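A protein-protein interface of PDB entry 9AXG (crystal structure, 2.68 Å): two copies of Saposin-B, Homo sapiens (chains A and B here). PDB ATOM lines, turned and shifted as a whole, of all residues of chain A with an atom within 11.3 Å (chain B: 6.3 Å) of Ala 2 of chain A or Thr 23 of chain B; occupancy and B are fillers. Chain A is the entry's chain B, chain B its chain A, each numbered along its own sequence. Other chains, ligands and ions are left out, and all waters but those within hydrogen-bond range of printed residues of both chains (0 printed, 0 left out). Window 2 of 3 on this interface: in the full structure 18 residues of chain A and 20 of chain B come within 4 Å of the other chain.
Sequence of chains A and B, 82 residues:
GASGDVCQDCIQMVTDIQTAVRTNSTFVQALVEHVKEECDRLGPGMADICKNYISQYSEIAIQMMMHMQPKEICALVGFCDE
The side-chain carboxylate (OD2) of Asp 16 of chain B lies close to the side-chain carboxylate (OD1) of Asp 9 of chain A (2.8 Å).
The side-chain sulfur (SG) of Cys 7 of chain A is disulfide-bonded to the side-chain sulfur (SG) of Cys 80 of chain A (2.0 Å). OD1 of Asp 5 of chain A sits close to OE1 of Gln 8 of chain A (3.5 Å). OG1 of Thr 23 of chain B lies close to O of Thr 19 of chain B. The side-chain amide oxygen (OD1) of Asn 24 of chain B sits at hydrogen-bond distance from the backbone NH (N) of Phe 27 of chain B, 3.4 Å away.
Among the printed residues, merely in contact across the chains: Ala 2 of chain A with Ala 20 of chain B (3.8 Å), Ala 2 of chain A with Thr 23 of chain B (3.5 Å), Ser 3 of chain A with Phe 27 of chain B (3.8 Å), Asp 5 of chain A with Asp 16 of chain B (3.4 Å), Val 6 of chain A with Asp 16 of chain B (3.4 Å), Val 6 of chain A with Ile 17 of chain B (3.7 Å) and Phe 79 of chain A with Ile 17 of chain B (3.7 Å).
Printed residues of chain B that touch a printed residue of chain A: Asp 16, Ile 17, Ala 20, Thr 23 and Phe 27. Hydrophobic or aromatic side chains of chain B that line the printed part of chain A: Ile 17 and Phe 27. Of the 14 printed residues of chain A, 6 touch a printed residue of chain B. Printed residues of chain A that touch a printed residue of chain B: Ala 2, Ser 3, Asp 5, Val 6, Asp 9 and Phe 79.
No position is printed for both chains. Of the 8 pairs that touch across the chains among the printed residues, none has its exchanged pair printed and touching as well.
Ala 2 of chain A touches two residues of chain B. Of the printed residues of chain B, Ser 3 of chain A touches Phe 27. Of the printed residues of chain B, Asp 5 of chain A touches Asp 16 (3.4 Å). Of the printed residues of chain B, Val 6 of chain A touches Asp 16 and Ile 17. Of the printed residues of chain B, Phe 79 of chain A touches Ile 17 (3.7 Å). Of the printed residues of chain A, Asp 16 of chain B touches Asp 5, Val 6 and Asp 9. Of the printed residues of chain A, Ala 20 of chain B touches Ala 2 (3.8 Å). No residue of chain A comes within 4 Å of Val 21 of chain B. No residue of chain A comes within 4 Å of Ser 25 of chain B. Of the printed residues of chain A, Phe 27 of chain B touches Ser 3 (3.8 Å).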
ATOM      1  N   GLY A   1      -9.244  -7.825 -12.861  1.00  0.00           N
ATOM      2  CA  GLY A   1      -8.724  -6.486 -13.080  1.00  0.00           C
ATOM      3  C   GLY A   1      -8.128  -5.829 -11.845  1.00  0.00           C
ATOM      4  O   GLY A   1      -7.288  -6.416 -11.164  1.00  0.00           O
ATOM      5  N   ALA A   2      -8.576  -4.604 -11.556  1.00  0.00           N
ATOM      6  CA  ALA A   2      -7.991  -3.831 -10.464  1.00  0.00           C
ATOM      7  C   ALA A   2      -8.413  -4.372  -9.100  1.00  0.00           C
ATOM      8  O   ALA A   2      -7.616  -4.372  -8.153  1.00  0.00           O
ATOM      9  CB  ALA A   2      -8.375  -2.357 -10.604  1.00  0.00           C
ATOM     10  N   SER A   3      -9.663  -4.820  -8.975  1.00  0.00           N
ATOM     11  CA  SER A   3     -10.140  -5.367  -7.709  1.00  0.00           C
ATOM     12  C   SER A   3      -9.627  -6.784  -7.458  1.00  0.00           C
ATOM     13  O   SER A   3      -9.483  -7.184  -6.297  1.00  0.00           O
ATOM     14  CB  SER A   3     -11.671  -5.321  -7.672  1.00  0.00           C
ATOM     15  OG  SER A   3     -12.243  -6.557  -8.059  1.00  0.00           O
ATOM     16  N   GLY A   4      -9.367  -7.560  -8.518  1.00  0.00           N
ATOM     17  CA  GLY A   4      -8.734  -8.859  -8.346  1.00  0.00           C
ATOM     18  C   GLY A   4      -7.303  -8.758  -7.856  1.00  0.00           C
ATOM     19  O   GLY A   4      -6.849  -9.598  -7.066  1.00  0.00           O
ATOM     20  N   ASP A   5      -6.580  -7.728  -8.315  1.00  0.00           N
ATOM     21  CA  ASP A   5      -5.255  -7.427  -7.789  1.00  0.00           C
ATOM     22  C   ASP A   5      -5.314  -7.106  -6.305  1.00  0.00           C
ATOM     23  O   ASP A   5      -4.429  -7.513  -5.545  1.00  0.00           O
ATOM     24  CB  ASP A   5      -4.639  -6.259  -8.555  1.00  0.00           C
ATOM     25  CG  ASP A   5      -4.178  -6.648  -9.940  1.00  0.00           C
ATOM     26  OD1 ASP A   5      -4.103  -7.860 -10.230  1.00  0.00           O
ATOM     27  OD2 ASP A   5      -3.875  -5.739 -10.738  1.00  0.00           O
ATOM     28  N   VAL A   6      -6.362  -6.396  -5.874  1.00  0.00           N
ATOM     29  CA  VAL A   6      -6.551  -6.075  -4.461  1.00  0.00           C
ATOM     30  C   VAL A   6      -6.766  -7.349  -3.644  1.00  0.00           C
ATOM     31  O   VAL A   6      -6.194  -7.511  -2.556  1.00  0.00           O
ATOM     32  CB  VAL A   6      -7.723  -5.083  -4.306  1.00  0.00           C
ATOM     33  CG1 VAL A   6      -8.144  -4.936  -2.846  1.00  0.00           C
ATOM     34  CG2 VAL A   6      -7.365  -3.732  -4.910  1.00  0.00           C
ATOM     35  N   CYS A   7      -7.561  -8.284  -4.177  1.00  0.00           N
ATOM     36  CA  CYS A   7      -7.784  -9.576  -3.525  1.00  0.00           C
ATOM     37  C   CYS A   7      -6.486 -10.363  -3.382  1.00  0.00           C
ATOM     38  O   CYS A   7      -6.192 -10.891  -2.303  1.00  0.00           O
ATOM     39  CB  CYS A   7      -8.810 -10.385  -4.325  1.00  0.00           C
ATOM     40  SG  CYS A   7      -9.226 -12.046  -3.669  1.00  0.00           S
ATOM     41  N   GLN A   8      -5.683 -10.419  -4.461  1.00  0.00           N
ATOM     42  CA  GLN A   8      -4.389 -11.100  -4.414  1.00  0.00           C
ATOM     43  C   GLN A   8      -3.461 -10.471  -3.378  1.00  0.00           C
ATOM     44  O   GLN A   8      -2.841 -11.186  -2.567  1.00  0.00           O
ATOM     45  CB  GLN A   8      -3.737 -11.072  -5.797  1.00  0.00           C
ATOM     46  CG  GLN A   8      -4.327 -12.075  -6.779  1.00  0.00           C
ATOM     47  CD  GLN A   8      -4.175 -11.660  -8.221  1.00  0.00           C
ATOM     48  OE1 GLN A   8      -3.328 -10.831  -8.556  1.00  0.00           O
ATOM     49  NE2 GLN A   8      -5.008 -12.231  -9.091  1.00  0.00           N
ATOM     50  N   ASP A   9      -3.399  -9.130  -3.365  1.00  0.00           N
ATOM     51  CA  ASP A   9      -2.573  -8.403  -2.404  1.00  0.00           C
ATOM     52  C   ASP A   9      -3.010  -8.679  -0.972  1.00  0.00           C
ATOM     53  O   ASP A   9      -2.169  -8.797  -0.071  1.00  0.00           O
ATOM     54  CB  ASP A   9      -2.648  -6.901  -2.667  1.00  0.00           C
ATOM     55  CG  ASP A   9      -2.029  -6.478  -3.970  1.00  0.00           C
ATOM     56  OD1 ASP A   9      -2.177  -5.289  -4.308  1.00  0.00           O
ATOM     57  OD2 ASP A   9      -1.391  -7.300  -4.644  1.00  0.00           O
ATOM     58  N   CYS A  10      -4.327  -8.782  -0.752  1.00  0.00           N
ATOM     59  CA  CYS A  10      -4.848  -9.077   0.576  1.00  0.00           C
ATOM     60  C   CYS A  10      -4.446 -10.467   1.039  1.00  0.00           C
ATOM     61  O   CYS A  10      -4.065 -10.631   2.203  1.00  0.00           O
ATOM     62  CB  CYS A  10      -6.371  -8.941   0.611  1.00  0.00           C
ATOM     63  SG  CYS A  10      -7.074  -9.177   2.281  1.00  0.00           S
ATOM     64  N   GLY A  78     -13.828  -7.588   2.783  1.00  0.00           N
ATOM     65  CA  GLY A  78     -14.413  -7.149   1.532  1.00  0.00           C
ATOM     66  C   GLY A  78     -13.473  -7.071   0.348  1.00  0.00           C
ATOM     67  O   GLY A  78     -13.936  -6.794  -0.767  1.00  0.00           O
ATOM     68  N   PHE A  79     -12.177  -7.316   0.542  1.00  0.00           N
ATOM     69  CA  PHE A  79     -11.243  -7.262  -0.575  1.00  0.00           C
ATOM     70  C   PHE A  79     -11.323  -8.490  -1.466  1.00  0.00           C
ATOM     71  O   PHE A  79     -10.800  -8.452  -2.584  1.00  0.00           O
ATOM     72  CB  PHE A  79      -9.811  -7.093  -0.068  1.00  0.00           C
ATOM     73  CG  PHE A  79      -9.570  -5.786   0.622  1.00  0.00           C
ATOM     74  CD1 PHE A  79     -10.230  -4.638   0.215  1.00  0.00           C
ATOM     75  CD2 PHE A  79      -8.706  -5.711   1.697  1.00  0.00           C
ATOM     76  CE1 PHE A  79     -10.016  -3.428   0.859  1.00  0.00           C
ATOM     77  CE2 PHE A  79      -8.492  -4.509   2.355  1.00  0.00           C
ATOM     78  CZ  PHE A  79      -9.147  -3.366   1.934  1.00  0.00           C
ATOM     79  N   CYS A  80     -11.964  -9.571  -1.016  1.00  0.00           N
ATOM     80  CA  CYS A  80     -12.146 -10.748  -1.857  1.00  0.00           C
ATOM     81  C   CYS A  80     -13.610 -11.152  -1.881  1.00  0.00           C
ATOM     82  O   CYS A  80     -14.380 -10.825  -0.972  1.00  0.00           O
ATOM     83  CB  CYS A  80     -11.300 -11.946  -1.395  1.00  0.00           C
ATOM     84  SG  CYS A  80      -9.516 -11.760  -1.676  1.00  0.00           S
ATOM     85  N   ASP A  81     -13.957 -11.883  -2.945  1.00  0.00           N
ATOM     86  CA  ASP A  81     -15.315 -12.316  -3.281  1.00  0.00           C
ATOM     87  C   ASP A  81     -16.237 -11.102  -3.417  1.00  0.00           C
ATOM     88  O   ASP A  81     -16.323 -10.524  -4.504  1.00  0.00           O
ATOM     89  CB  ASP A  81     -15.847 -13.326  -2.245  1.00  0.00           C
ATOM     90  CG  ASP A  81     -14.887 -14.498  -2.020  1.00  0.00           C
ATOM     91  OD1 ASP A  81     -13.938 -14.667  -2.819  1.00  0.00           O
ATOM     92  OD2 ASP A  81     -15.077 -15.247  -1.035  1.00  0.00           O
ATOM     93  N   ASP B  16      -2.771  -0.776  -5.203  1.00  0.00           N
ATOM     94  CA  ASP B  16      -3.820  -1.340  -6.044  1.00  0.00           C
ATOM     95  C   ASP B  16      -5.224  -0.962  -5.584  1.00  0.00           C
ATOM     96  O   ASP B  16      -6.144  -0.962  -6.406  1.00  0.00           O
ATOM     97  CB  ASP B  16      -3.685  -2.853  -6.119  1.00  0.00           C
ATOM     98  CG  ASP B  16      -2.501  -3.272  -6.942  1.00  0.00           C
ATOM     99  OD1 ASP B  16      -1.908  -2.397  -7.609  1.00  0.00           O
ATOM    100  OD2 ASP B  16      -2.190  -4.476  -6.970  1.00  0.00           O
ATOM    101  N   ILE B  17      -5.411  -0.615  -4.309  1.00  0.00           N
ATOM    102  CA  ILE B  17      -6.713  -0.129  -3.863  1.00  0.00           C
ATOM    103  C   ILE B  17      -6.994   1.253  -4.444  1.00  0.00           C
ATOM    104  O   ILE B  17      -8.097   1.516  -4.941  1.00  0.00           O
ATOM    105  CB  ILE B  17      -6.786  -0.139  -2.326  1.00  0.00           C
ATOM    106  CG1 ILE B  17      -7.092  -1.546  -1.825  1.00  0.00           C
ATOM    107  CG2 ILE B  17      -7.867   0.790  -1.819  1.00  0.00           C
ATOM    108  CD1 ILE B  17      -6.700  -1.773  -0.382  1.00  0.00           C
ATOM    109  N   GLN B  18      -5.996   2.147  -4.411  1.00  0.00           N
ATOM    110  CA  GLN B  18      -6.143   3.465  -5.031  1.00  0.00           C
ATOM    111  C   GLN B  18      -6.338   3.343  -6.540  1.00  0.00           C
ATOM    112  O   GLN B  18      -7.111   4.108  -7.140  1.00  0.00           O
ATOM    113  CB  GLN B  18      -4.926   4.338  -4.708  1.00  0.00           C
ATOM    114  CG  GLN B  18      -4.778   4.639  -3.214  1.00  0.00           C
ATOM    115  CD  GLN B  18      -3.559   5.484  -2.868  1.00  0.00           C
ATOM    116  OE1 GLN B  18      -2.598   5.572  -3.634  1.00  0.00           O
ATOM    117  NE2 GLN B  18      -3.602   6.117  -1.705  1.00  0.00           N
ATOM    118  N   THR B  19      -5.675   2.358  -7.159  1.00  0.00           N
ATOM    119  CA  THR B  19      -5.941   2.047  -8.559  1.00  0.00           C
ATOM    120  C   THR B  19      -7.386   1.591  -8.760  1.00  0.00           C
ATOM    121  O   THR B  19      -8.054   2.032  -9.700  1.00  0.00           O
ATOM    122  CB  THR B  19      -4.964   0.977  -9.053  1.00  0.00           C
ATOM    123  OG1 THR B  19      -3.610   1.394  -8.801  1.00  0.00           O
ATOM    124  CG2 THR B  19      -5.139   0.738 -10.545  1.00  0.00           C
ATOM    125  N   ALA B  20      -7.898   0.745  -7.860  1.00  0.00           N
ATOM    126  CA  ALA B  20      -9.267   0.252  -7.987  1.00  0.00           C
ATOM    127  C   ALA B  20     -10.287   1.368  -7.805  1.00  0.00           C
ATOM    128  O   ALA B  20     -11.318   1.385  -8.482  1.00  0.00           O
ATOM    129  CB  ALA B  20      -9.521  -0.867  -6.981  1.00  0.00           C
ATOM    130  N   VAL B  21     -10.012   2.311  -6.905  1.00  0.00           N
ATOM    131  CA  VAL B  21     -10.910   3.447  -6.722  1.00  0.00           C
ATOM    132  C   VAL B  21     -10.868   4.359  -7.946  1.00  0.00           C
ATOM    133  O   VAL B  21     -11.900   4.894  -8.369  1.00  0.00           O
ATOM    134  CB  VAL B  21     -10.573   4.197  -5.419  1.00  0.00           C
ATOM    135  CG1 VAL B  21     -11.434   5.444  -5.238  1.00  0.00           C
ATOM    136  CG2 VAL B  21     -10.752   3.291  -4.214  1.00  0.00           C
ATOM    137  N   ARG B  22      -9.691   4.512  -8.569  1.00  0.00           N
ATOM    138  CA  ARG B  22      -9.612   5.358  -9.762  1.00  0.00           C
ATOM    139  C   ARG B  22     -10.287   4.715 -10.977  1.00  0.00           C
ATOM    140  O   ARG B  22     -10.958   5.410 -11.751  1.00  0.00           O
ATOM    141  CB  ARG B  22      -8.153   5.716 -10.071  1.00  0.00           C
ATOM    142  CG  ARG B  22      -7.687   6.999  -9.375  1.00  0.00           C
ATOM    143  CD  ARG B  22      -6.284   6.867  -8.795  1.00  0.00           C
ATOM    144  NE  ARG B  22      -5.726   8.146  -8.367  1.00  0.00           N
ATOM    145  CZ  ARG B  22      -4.853   8.283  -7.376  1.00  0.00           C
ATOM    146  NH1 ARG B  22      -4.417   7.238  -6.691  1.00  0.00           N
ATOM    147  NH2 ARG B  22      -4.404   9.497  -7.065  1.00  0.00           N
ATOM    148  N   THR B  23     -10.139   3.403 -11.164  1.00  0.00           N
ATOM    149  CA  THR B  23     -10.626   2.747 -12.378  1.00  0.00           C
ATOM    150  C   THR B  23     -11.982   2.059 -12.238  1.00  0.00           C
ATOM    151  O   THR B  23     -12.750   2.046 -13.207  1.00  0.00           O
ATOM    152  CB  THR B  23      -9.591   1.731 -12.890  1.00  0.00           C
ATOM    153  OG1 THR B  23      -9.684   0.505 -12.141  1.00  0.00           O
ATOM    154  CG2 THR B  23      -8.173   2.302 -12.872  1.00  0.00           C
ATOM    155  N   ASN B  24     -12.308   1.481 -11.085  1.00  0.00           N
ATOM    156  CA  ASN B  24     -13.559   0.747 -10.915  1.00  0.00           C
ATOM    157  C   ASN B  24     -14.561   1.655 -10.208  1.00  0.00           C
ATOM    158  O   ASN B  24     -14.347   2.045  -9.054  1.00  0.00           O
ATOM    159  CB  ASN B  24     -13.321  -0.542 -10.124  1.00  0.00           C
ATOM    160  CG  ASN B  24     -14.478  -1.534 -10.210  1.00  0.00           C
ATOM    161  OD1 ASN B  24     -15.653  -1.163 -10.314  1.00  0.00           O
ATOM    162  ND2 ASN B  24     -14.140  -2.820 -10.119  1.00  0.00           N
ATOM    163  N   SER B  25     -15.662   1.966 -10.896  1.00  0.00           N
ATOM    164  CA  SER B  25     -16.672   2.859 -10.341  1.00  0.00           C
ATOM    165  C   SER B  25     -17.481   2.200  -9.235  1.00  0.00           C
ATOM    166  O   SER B  25     -17.987   2.893  -8.345  1.00  0.00           O
ATOM    167  CB  SER B  25     -17.610   3.339 -11.450  1.00  0.00           C
ATOM    168  OG  SER B  25     -17.827   2.318 -12.406  1.00  0.00           O
ATOM    169  N   PHE B  27     -16.279  -0.214  -7.132  1.00  0.00           N
ATOM    170  CA  PHE B  27     -15.403  -0.846  -6.141  1.00  0.00           C
ATOM    171  C   PHE B  27     -15.708  -0.356  -4.727  1.00  0.00           C
ATOM    172  O   PHE B  27     -15.870  -1.160  -3.795  1.00  0.00           O
ATOM    173  CB  PHE B  27     -13.942  -0.563  -6.501  1.00  0.00           C
ATOM    174  CG  PHE B  27     -12.940  -1.045  -5.479  1.00  0.00           C
ATOM    175  CD1 PHE B  27     -12.609  -2.389  -5.387  1.00  0.00           C
ATOM    176  CD2 PHE B  27     -12.311  -0.148  -4.625  1.00  0.00           C
ATOM    177  CE1 PHE B  27     -11.682  -2.833  -4.455  1.00  0.00           C
ATOM    178  CE2 PHE B  27     -11.377  -0.590  -3.683  1.00  0.00           C
ATOM    179  CZ  PHE B  27     -11.066  -1.933  -3.603  1.00  0.00           C
